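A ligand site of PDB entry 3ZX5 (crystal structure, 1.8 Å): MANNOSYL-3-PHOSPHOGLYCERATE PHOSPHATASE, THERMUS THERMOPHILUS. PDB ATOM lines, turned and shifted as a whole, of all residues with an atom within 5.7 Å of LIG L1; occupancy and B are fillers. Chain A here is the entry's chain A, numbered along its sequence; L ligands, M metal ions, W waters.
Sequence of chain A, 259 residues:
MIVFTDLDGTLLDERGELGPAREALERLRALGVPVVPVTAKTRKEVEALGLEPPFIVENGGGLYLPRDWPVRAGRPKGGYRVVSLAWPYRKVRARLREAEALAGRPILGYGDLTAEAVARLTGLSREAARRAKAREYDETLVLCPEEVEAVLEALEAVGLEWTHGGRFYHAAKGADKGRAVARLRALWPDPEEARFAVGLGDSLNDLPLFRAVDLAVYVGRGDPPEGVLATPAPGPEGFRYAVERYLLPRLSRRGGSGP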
ATOM      1  N   ASP A   6      25.697  23.249 -25.592  1.00  0.00           N
ATOM      2  CA  ASP A   6      25.751  22.059 -24.786  1.00  0.00           C
ATOM      3  C   ASP A   6      24.749  21.058 -25.375  1.00  0.00           C
ATOM      4  O   ASP A   6      23.845  21.450 -26.122  1.00  0.00           O
ATOM      5  CB  ASP A   6      25.394  22.436 -23.354  1.00  0.00           C
ATOM      6  CG  ASP A   6      25.218  21.256 -22.455  1.00  0.00           C
ATOM      7  OD1 ASP A   6      26.086  20.363 -22.405  1.00  0.00           O
ATOM      8  OD2 ASP A   6      24.169  21.234 -21.792  1.00  0.00           O
ATOM      9  N   ASP A   8      23.358  17.486 -23.598  1.00  0.00           N
ATOM     10  CA  ASP A   8      22.393  16.977 -22.614  1.00  0.00           C
ATOM     11  C   ASP A   8      21.612  18.121 -21.981  1.00  0.00           C
ATOM     12  O   ASP A   8      22.197  19.044 -21.454  1.00  0.00           O
ATOM     13  CB  ASP A   8      23.114  16.227 -21.491  1.00  0.00           C
ATOM     14  CG  ASP A   8      23.710  14.910 -21.960  1.00  0.00           C
ATOM     15  OD1 ASP A   8      23.089  14.232 -22.803  1.00  0.00           O
ATOM     16  OD2 ASP A   8      24.807  14.562 -21.473  1.00  0.00           O
ATOM     17  N   ALA A  40      30.132  17.628 -22.193  1.00  0.00           N
ATOM     18  CA  ALA A  40      30.871  16.691 -21.339  1.00  0.00           C
ATOM     19  C   ALA A  40      31.012  15.348 -22.038  1.00  0.00           C
ATOM     20  O   ALA A  40      31.825  14.501 -21.639  1.00  0.00           O
ATOM     21  CB  ALA A  40      30.145  16.508 -19.983  1.00  0.00           C
ATOM     22  N   LYS A  41      30.226  15.141 -23.087  1.00  0.00           N
ATOM     23  CA  LYS A  41      30.235  13.854 -23.783  1.00  0.00           C
ATOM     24  C   LYS A  41      31.565  13.580 -24.497  1.00  0.00           C
ATOM     25  O   LYS A  41      32.331  14.501 -24.790  1.00  0.00           O
ATOM     26  CB  LYS A  41      29.047  13.762 -24.772  1.00  0.00           C
ATOM     27  CG  LYS A  41      27.682  13.681 -24.079  1.00  0.00           C
ATOM     28  CD  LYS A  41      26.515  13.797 -25.056  1.00  0.00           C
ATOM     29  CE  LYS A  41      25.548  12.618 -24.952  1.00  0.00           C
ATOM     30  NZ  LYS A  41      24.989  12.444 -23.559  1.00  0.00           N
ATOM     31  N   THR A  42      31.848  12.309 -24.743  1.00  0.00           N
ATOM     32  CA  THR A  42      33.075  11.937 -25.438  1.00  0.00           C
ATOM     33  C   THR A  42      32.892  12.093 -26.949  1.00  0.00           C
ATOM     34  O   THR A  42      31.765  12.200 -27.438  1.00  0.00           O
ATOM     35  CB  THR A  42      33.457  10.467 -25.206  1.00  0.00           C
ATOM     36  OG1 THR A  42      32.493   9.625 -25.861  1.00  0.00           O
ATOM     37  CG2 THR A  42      33.503  10.145 -23.695  1.00  0.00           C
ATOM     38  N   GLU A  45      30.620   9.549 -28.413  1.00  0.00           N
ATOM     39  CA  GLU A  45      29.215   9.875 -28.243  1.00  0.00           C
ATOM     40  C   GLU A  45      28.747  10.909 -29.269  1.00  0.00           C
ATOM     41  O   GLU A  45      27.687  10.777 -29.869  1.00  0.00           O
ATOM     42  CB  GLU A  45      28.951  10.371 -26.828  1.00  0.00           C
ATOM     43  CG  GLU A  45      29.117   9.316 -25.748  1.00  0.00           C
ATOM     44  CD  GLU A  45      28.845   9.865 -24.363  1.00  0.00           C
ATOM     45  OE1 GLU A  45      29.699  10.608 -23.821  1.00  0.00           O
ATOM     46  OE2 GLU A  45      27.760   9.565 -23.811  1.00  0.00           O
ATOM     47  N   TYR A 110      33.449   6.131 -14.008  1.00  0.00           N
ATOM     48  CA  TYR A 110      33.157   5.253 -15.127  1.00  0.00           C
ATOM     49  C   TYR A 110      34.274   4.255 -15.383  1.00  0.00           C
ATOM     50  O   TYR A 110      34.005   3.112 -15.760  1.00  0.00           O
ATOM     51  CB  TYR A 110      32.965   6.053 -16.410  1.00  0.00           C
ATOM     52  CG  TYR A 110      31.663   6.786 -16.565  1.00  0.00           C
ATOM     53  CD1 TYR A 110      30.770   6.920 -15.506  1.00  0.00           C
ATOM     54  CD2 TYR A 110      31.320   7.335 -17.791  1.00  0.00           C
ATOM     55  CE1 TYR A 110      29.557   7.600 -15.676  1.00  0.00           C
ATOM     56  CE2 TYR A 110      30.137   8.023 -17.967  1.00  0.00           C
ATOM     57  CZ  TYR A 110      29.264   8.162 -16.915  1.00  0.00           C
ATOM     58  OH  TYR A 110      28.101   8.860 -17.112  1.00  0.00           O
ATOM     59  N   THR A 122      22.943   5.598 -15.942  1.00  0.00           N
ATOM     60  CA  THR A 122      22.694   6.746 -16.813  1.00  0.00           C
ATOM     61  C   THR A 122      21.405   6.644 -17.628  1.00  0.00           C
ATOM     62  O   THR A 122      20.942   7.632 -18.196  1.00  0.00           O
ATOM     63  CB  THR A 122      23.820   6.932 -17.836  1.00  0.00           C
ATOM     64  OG1 THR A 122      23.876   5.775 -18.671  1.00  0.00           O
ATOM     65  CG2 THR A 122      25.171   7.149 -17.130  1.00  0.00           C
ATOM     66  N   LEU A 124      21.353   5.070 -20.286  1.00  0.00           N
ATOM     67  CA  LEU A 124      21.827   4.814 -21.643  1.00  0.00           C
ATOM     68  C   LEU A 124      21.775   3.319 -21.960  1.00  0.00           C
ATOM     69  O   LEU A 124      21.724   2.489 -21.050  1.00  0.00           O
ATOM     70  CB  LEU A 124      23.263   5.302 -21.816  1.00  0.00           C
ATOM     71  CG  LEU A 124      23.549   6.795 -21.658  1.00  0.00           C
ATOM     72  CD1 LEU A 124      25.054   7.014 -21.521  1.00  0.00           C
ATOM     73  CD2 LEU A 124      22.961   7.576 -22.825  1.00  0.00           C
ATOM     74  N   ALA A 132      30.250   6.300 -23.776  1.00  0.00           N
ATOM     75  CA  ALA A 132      30.436   7.227 -22.666  1.00  0.00           C
ATOM     76  C   ALA A 132      31.672   6.874 -21.821  1.00  0.00           C
ATOM     77  O   ALA A 132      32.278   7.746 -21.186  1.00  0.00           O
ATOM     78  CB  ALA A 132      29.159   7.306 -21.778  1.00  0.00           C
ATOM     79  N   ARG A 135      36.609   7.648 -22.599  1.00  0.00           N
ATOM     80  CA  ARG A 135      36.988   8.986 -22.184  1.00  0.00           C
ATOM     81  C   ARG A 135      38.485   9.218 -22.334  1.00  0.00           C
ATOM     82  O   ARG A 135      39.306   8.380 -21.946  1.00  0.00           O
ATOM     83  CB  ARG A 135      36.527   9.244 -20.749  1.00  0.00           C
ATOM     84  CG  ARG A 135      35.088   8.795 -20.481  1.00  0.00           C
ATOM     85  CD  ARG A 135      34.526   9.373 -19.154  1.00  0.00           C
ATOM     86  NE  ARG A 135      34.225  10.795 -19.243  1.00  0.00           N
ATOM     87  CZ  ARG A 135      33.139  11.300 -19.833  1.00  0.00           C
ATOM     88  NH1 ARG A 135      32.248  10.502 -20.420  1.00  0.00           N
ATOM     89  NH2 ARG A 135      32.961  12.622 -19.859  1.00  0.00           N
ATOM     90  N   THR A 140      34.034  10.779 -15.373  1.00  0.00           N
ATOM     91  CA  THR A 140      32.732  10.980 -14.747  1.00  0.00           C
ATOM     92  C   THR A 140      32.709  10.192 -13.433  1.00  0.00           C
ATOM     93  O   THR A 140      32.954   8.978 -13.427  1.00  0.00           O
ATOM     94  CB  THR A 140      31.573  10.544 -15.680  1.00  0.00           C
ATOM     95  OG1 THR A 140      31.719  11.185 -16.959  1.00  0.00           O
ATOM     96  CG2 THR A 140      30.225  10.918 -15.091  1.00  0.00           C
ATOM     97  N   HIS A 164      30.212  19.862 -12.478  1.00  0.00           N
ATOM     98  CA  HIS A 164      29.179  18.864 -12.676  1.00  0.00           C
ATOM     99  C   HIS A 164      28.265  19.227 -13.837  1.00  0.00           C
ATOM    100  O   HIS A 164      28.074  20.408 -14.133  1.00  0.00           O
ATOM    101  CB  HIS A 164      28.387  18.570 -11.387  1.00  0.00           C
ATOM    102  CG  HIS A 164      27.415  19.632 -10.999  1.00  0.00           C
ATOM    103  ND1 HIS A 164      26.218  19.817 -11.649  1.00  0.00           N
ATOM    104  CD2 HIS A 164      27.443  20.546  -9.998  1.00  0.00           C
ATOM    105  CE1 HIS A 164      25.557  20.819 -11.081  1.00  0.00           C
ATOM    106  NE2 HIS A 164      26.276  21.274 -10.065  1.00  0.00           N
ATOM    107  N   GLY A 165      27.769  18.206 -14.514  1.00  0.00           N
ATOM    108  CA  GLY A 165      26.821  18.396 -15.593  1.00  0.00           C
ATOM    109  C   GLY A 165      25.417  18.287 -15.041  1.00  0.00           C
ATOM    110  O   GLY A 165      25.168  18.683 -13.903  1.00  0.00           O
ATOM    111  N   GLY A 166      24.506  17.712 -15.814  1.00  0.00           N
ATOM    112  CA  GLY A 166      23.133  17.630 -15.361  1.00  0.00           C
ATOM    113  C   GLY A 166      22.988  16.718 -14.154  1.00  0.00           C
ATOM    114  O   GLY A 166      22.186  16.983 -13.246  1.00  0.00           O
ATOM    115  N   ARG A 167      23.762  15.640 -14.130  1.00  0.00           N
ATOM    116  CA  ARG A 167      23.568  14.604 -13.121  1.00  0.00           C
ATOM    117  C   ARG A 167      24.840  14.148 -12.416  1.00  0.00           C
ATOM    118  O   ARG A 167      24.781  13.698 -11.277  1.00  0.00           O
ATOM    119  CB  ARG A 167      22.850  13.399 -13.737  1.00  0.00           C
ATOM    120  CG  ARG A 167      21.439  13.715 -14.213  1.00  0.00           C
ATOM    121  CD  ARG A 167      20.752  12.452 -14.694  1.00  0.00           C
ATOM    122  NE  ARG A 167      21.415  11.878 -15.858  1.00  0.00           N
ATOM    123  CZ  ARG A 167      21.084  10.714 -16.395  1.00  0.00           C
ATOM    124  NH1 ARG A 167      20.096  10.010 -15.880  1.00  0.00           N
ATOM    125  NH2 ARG A 167      21.741  10.260 -17.459  1.00  0.00           N
ATOM    126  N   PHE A 168      25.974  14.280 -13.085  1.00  0.00           N
ATOM    127  CA  PHE A 168      27.216  13.730 -12.551  1.00  0.00           C
ATOM    128  C   PHE A 168      28.320  14.753 -12.300  1.00  0.00           C
ATOM    129  O   PHE A 168      28.455  15.752 -13.020  1.00  0.00           O
ATOM    130  CB  PHE A 168      27.752  12.645 -13.479  1.00  0.00           C
ATOM    131  CG  PHE A 168      26.819  11.469 -13.616  1.00  0.00           C
ATOM    132  CD1 PHE A 168      26.767  10.496 -12.637  1.00  0.00           C
ATOM    133  CD2 PHE A 168      25.993  11.348 -14.725  1.00  0.00           C
ATOM    134  CE1 PHE A 168      25.912   9.415 -12.754  1.00  0.00           C
ATOM    135  CE2 PHE A 168      25.126  10.272 -14.847  1.00  0.00           C
ATOM    136  CZ  PHE A 168      25.092   9.306 -13.866  1.00  0.00           C
ATOM    137  N   TYR A 169      29.121  14.486 -11.274  1.00  0.00           N
ATOM    138  CA  TYR A 169      30.346  15.228 -11.064  1.00  0.00           C
ATOM    139  C   TYR A 169      31.448  14.715 -11.980  1.00  0.00           C
ATOM    140  O   TYR A 169      31.443  13.546 -12.383  1.00  0.00           O
ATOM    141  CB  TYR A 169      30.783  15.131  -9.609  1.00  0.00           C
ATOM    142  CG  TYR A 169      29.991  16.056  -8.723  1.00  0.00           C
ATOM    143  CD1 TYR A 169      30.356  17.389  -8.579  1.00  0.00           C
ATOM    144  CD2 TYR A 169      28.863  15.595  -8.052  1.00  0.00           C
ATOM    145  CE1 TYR A 169      29.628  18.239  -7.793  1.00  0.00           C
ATOM    146  CE2 TYR A 169      28.130  16.451  -7.247  1.00  0.00           C
ATOM    147  CZ  TYR A 169      28.511  17.779  -7.130  1.00  0.00           C
ATOM    148  OH  TYR A 169      27.790  18.636  -6.334  1.00  0.00           O
ATOM    149  N   HIS A 170      32.377  15.597 -12.319  1.00  0.00           N
ATOM    150  CA  HIS A 170      33.476  15.242 -13.213  1.00  0.00           C
ATOM    151  C   HIS A 170      34.797  15.654 -12.590  1.00  0.00           C
ATOM    152  O   HIS A 170      34.846  16.598 -11.810  1.00  0.00           O
ATOM    153  CB  HIS A 170      33.329  15.951 -14.563  1.00  0.00           C
ATOM    154  CG  HIS A 170      32.147  15.483 -15.361  1.00  0.00           C
ATOM    155  ND1 HIS A 170      32.251  14.601 -16.406  1.00  0.00           N
ATOM    156  CD2 HIS A 170      30.822  15.760 -15.242  1.00  0.00           C
ATOM    157  CE1 HIS A 170      31.057  14.353 -16.913  1.00  0.00           C
ATOM    158  NE2 HIS A 170      30.171  15.057 -16.224  1.00  0.00           N
ATOM    159  N   SER A 203      23.598  23.773 -17.076  1.00  0.00           N
ATOM    160  CA  SER A 203      24.131  23.304 -15.799  1.00  0.00           C
ATOM    161  C   SER A 203      25.431  23.984 -15.420  1.00  0.00           C
ATOM    162  O   SER A 203      25.915  24.871 -16.116  1.00  0.00           O
ATOM    163  CB  SER A 203      24.340  21.790 -15.820  1.00  0.00           C
ATOM    164  OG  SER A 203      23.143  21.100 -16.095  1.00  0.00           O
ATOM    165  N   ASN A 205      28.527  23.077 -15.501  1.00  0.00           N
ATOM    166  CA  ASN A 205      29.644  22.972 -16.419  1.00  0.00           C
ATOM    167  C   ASN A 205      29.511  23.921 -17.618  1.00  0.00           C
ATOM    168  O   ASN A 205      30.438  24.059 -18.414  1.00  0.00           O
ATOM    169  CB  ASN A 205      29.883  21.516 -16.874  1.00  0.00           C
ATOM    170  CG  ASN A 205      28.712  20.938 -17.644  1.00  0.00           C
ATOM    171  OD1 ASN A 205      27.569  21.341 -17.468  1.00  0.00           O
ATOM    172  ND2 ASN A 205      29.003  19.958 -18.514  1.00  0.00           N
HETATM  173  C1  LIG L   1      27.924  12.679 -18.299  1.00  0.00           C
HETATM  174  O1  LIG L   1      27.683  14.003 -18.784  1.00  0.00           O
HETATM  175  C2  LIG L   1      26.482  14.626 -18.306  1.00  0.00           C
HETATM  176  C3  LIG L   1      26.364  16.011 -18.976  1.00  0.00           C
HETATM  177  O2  LIG L   1      25.227  16.707 -18.463  1.00  0.00           O
HETATM  178  C4  LIG L   1      26.473  14.750 -16.804  1.00  0.00           C
HETATM  179  O3  LIG L   1      27.474  15.204 -16.206  1.00  0.00           O
HETATM  180  O4  LIG L   1      25.365  14.682 -16.226  1.00  0.00           O
HETATM  181  C5  LIG L   1      29.057  12.068 -19.121  1.00  0.00           C
HETATM  182  O5  LIG L   1      29.472  10.807 -18.561  1.00  0.00           O
HETATM  183  C6  LIG L   1      28.595  11.861 -20.568  1.00  0.00           C
HETATM  184  O6  LIG L   1      29.634  11.247 -21.315  1.00  0.00           O
HETATM  185  C7  LIG L   1      27.366  10.969 -20.557  1.00  0.00           C
HETATM  186  O7  LIG L   1      26.824  10.867 -21.874  1.00  0.00           O
HETATM  187  C8  LIG L   1      26.270  11.527 -19.676  1.00  0.00           C
HETATM  188  C9  LIG L   1      25.132  10.500 -19.577  1.00  0.00           C
HETATM  189  O8  LIG L   1      23.969  11.150 -19.044  1.00  0.00           O
HETATM  190  O9  LIG L   1      26.735  11.895 -18.368  1.00  0.00           O
HETATM  191  V1  LG2 L   2      26.446  18.502 -21.638  1.00  0.00           V
HETATM  192  O1  LG2 L   2      28.166  18.907 -20.949  1.00  0.00           O
HETATM  193  O2  LG2 L   2      26.172  17.508 -23.212  1.00  0.00           O
HETATM  194  O3  LG2 L   2      25.067  18.464 -20.336  1.00  0.00           O
HETATM  195 MG    MG M   1      23.642  20.058 -20.136  1.00  0.00          MG
HETATM  196  O   HOH W   1      22.873  15.362 -18.367  1.00  0.00           O
HETATM  197  O   HOH W   2      23.518  12.878 -17.207  1.00  0.00           O
HETATM  198  O   HOH W   3      22.763  18.981 -18.424  1.00  0.00           O
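O3 of LIG L1 sits close to N of Gly 165.
The backbone NH of Phe 168 lies within hydrogen-bond range of an oxygen (O4) of LIG L1.
NH2 of Arg 167 is in hydrogen-bond range of O8 of LIG L1 (2.9 Å).
The side-chain hydroxyl of Thr 140 is in hydrogen-bond range of an oxygen (O5) of LIG L1.
A ring nitrogen (NE2) of His 170 is in hydrogen-bond range of an oxygen (O3) of LIG L1.
OD1 of Asp 6 binds V1 of LG2 L2 (2.0 Å).
The backbone NH of Arg 167 lies within hydrogen-bond range of an oxygen (O4) of LIG L1 (2.8 Å).
N of Ala 40 lies close to O1 of LG2 L2, 2.7 Å away.
An oxygen (O6) of LIG L1 sits at hydrogen-bond distance from the guanidinium group of Arg 135, at 2.9 Å.
O7 of LIG L1 sits at hydrogen-bond distance from NZ of Lys 41.
The backbone NH (N) of Gly 166 is in hydrogen-bond range of an oxygen (O2) of LIG L1 (2.9 Å).
The side-chain hydroxyl (OH) of Tyr 110 sits at hydrogen-bond distance from an oxygen (O5) of LIG L1 (2.8 Å).
OE2 of Glu 45 lies within hydrogen-bond range of O7 of LIG L1, at 2.5 Å.
Asp 8 touches LIG L1.
CB of Ala 40 touches O1 of LIG L1, 3.7 Å away.
CD1 of Leu 124 touches C9 of LIG L1 (3.99 Å).
CB of Ala 132 touches O6 of LIG L1 (3.996 Å).
Hydrophobic or aromatic side chains that line LIG L1: Ala 40, Tyr 110, Leu 124, Ala 132, Phe 168 and His 170.
Along chain A the residues within 4 Å of LIG L1 span positions 8 to 170.
The nearest printed residue that does not touch LIG L1 is Thr 122 (4.1 Å).
An oxygen (O3) of LG2 L2 sits close to an oxygen (O2) of LIG L1 (2.6 Å).
Water W2 lies within hydrogen-bond range of an oxygen (O8) of LIG L1 and the guanidinium group (NE) of Arg 167.
Water W3 lies within hydrogen-bond range of OG of Ser 203 (3.2 Å), O2 of LIG L1 (3.4 Å) and N of Gly 166 (3.4 Å).
O of Thr 122 sits at hydrogen-bond distance from NH2 of Arg 167, at 2.8 Å.
N of Thr 42 lies within hydrogen-bond range of OE1 of Glu 45 (2.9 Å).
The backbone NH of Leu 124 lies within hydrogen-bond range of the side-chain hydroxyl of Thr 122 (3.1 Å).
The side-chain carboxylate (OD1) of Asp 8 is in salt-bridge range of the side-chain amino group (NZ) of Lys 41 (2.7 Å).
NH2 of Arg 135 sits at hydrogen-bond distance from O of Ala 40 (2.8 Å).
N of Tyr 110 lies within hydrogen-bond range of O of Thr 140 (2.9 Å).
OG1 of Thr 140 sits close to NE of Arg 135, at 3.4 Å.
The guanidinium group (NH1) of Arg 135 is in hydrogen-bond range of the backbone carbonyl oxygen (O) of Ala 132 (2.9 Å).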
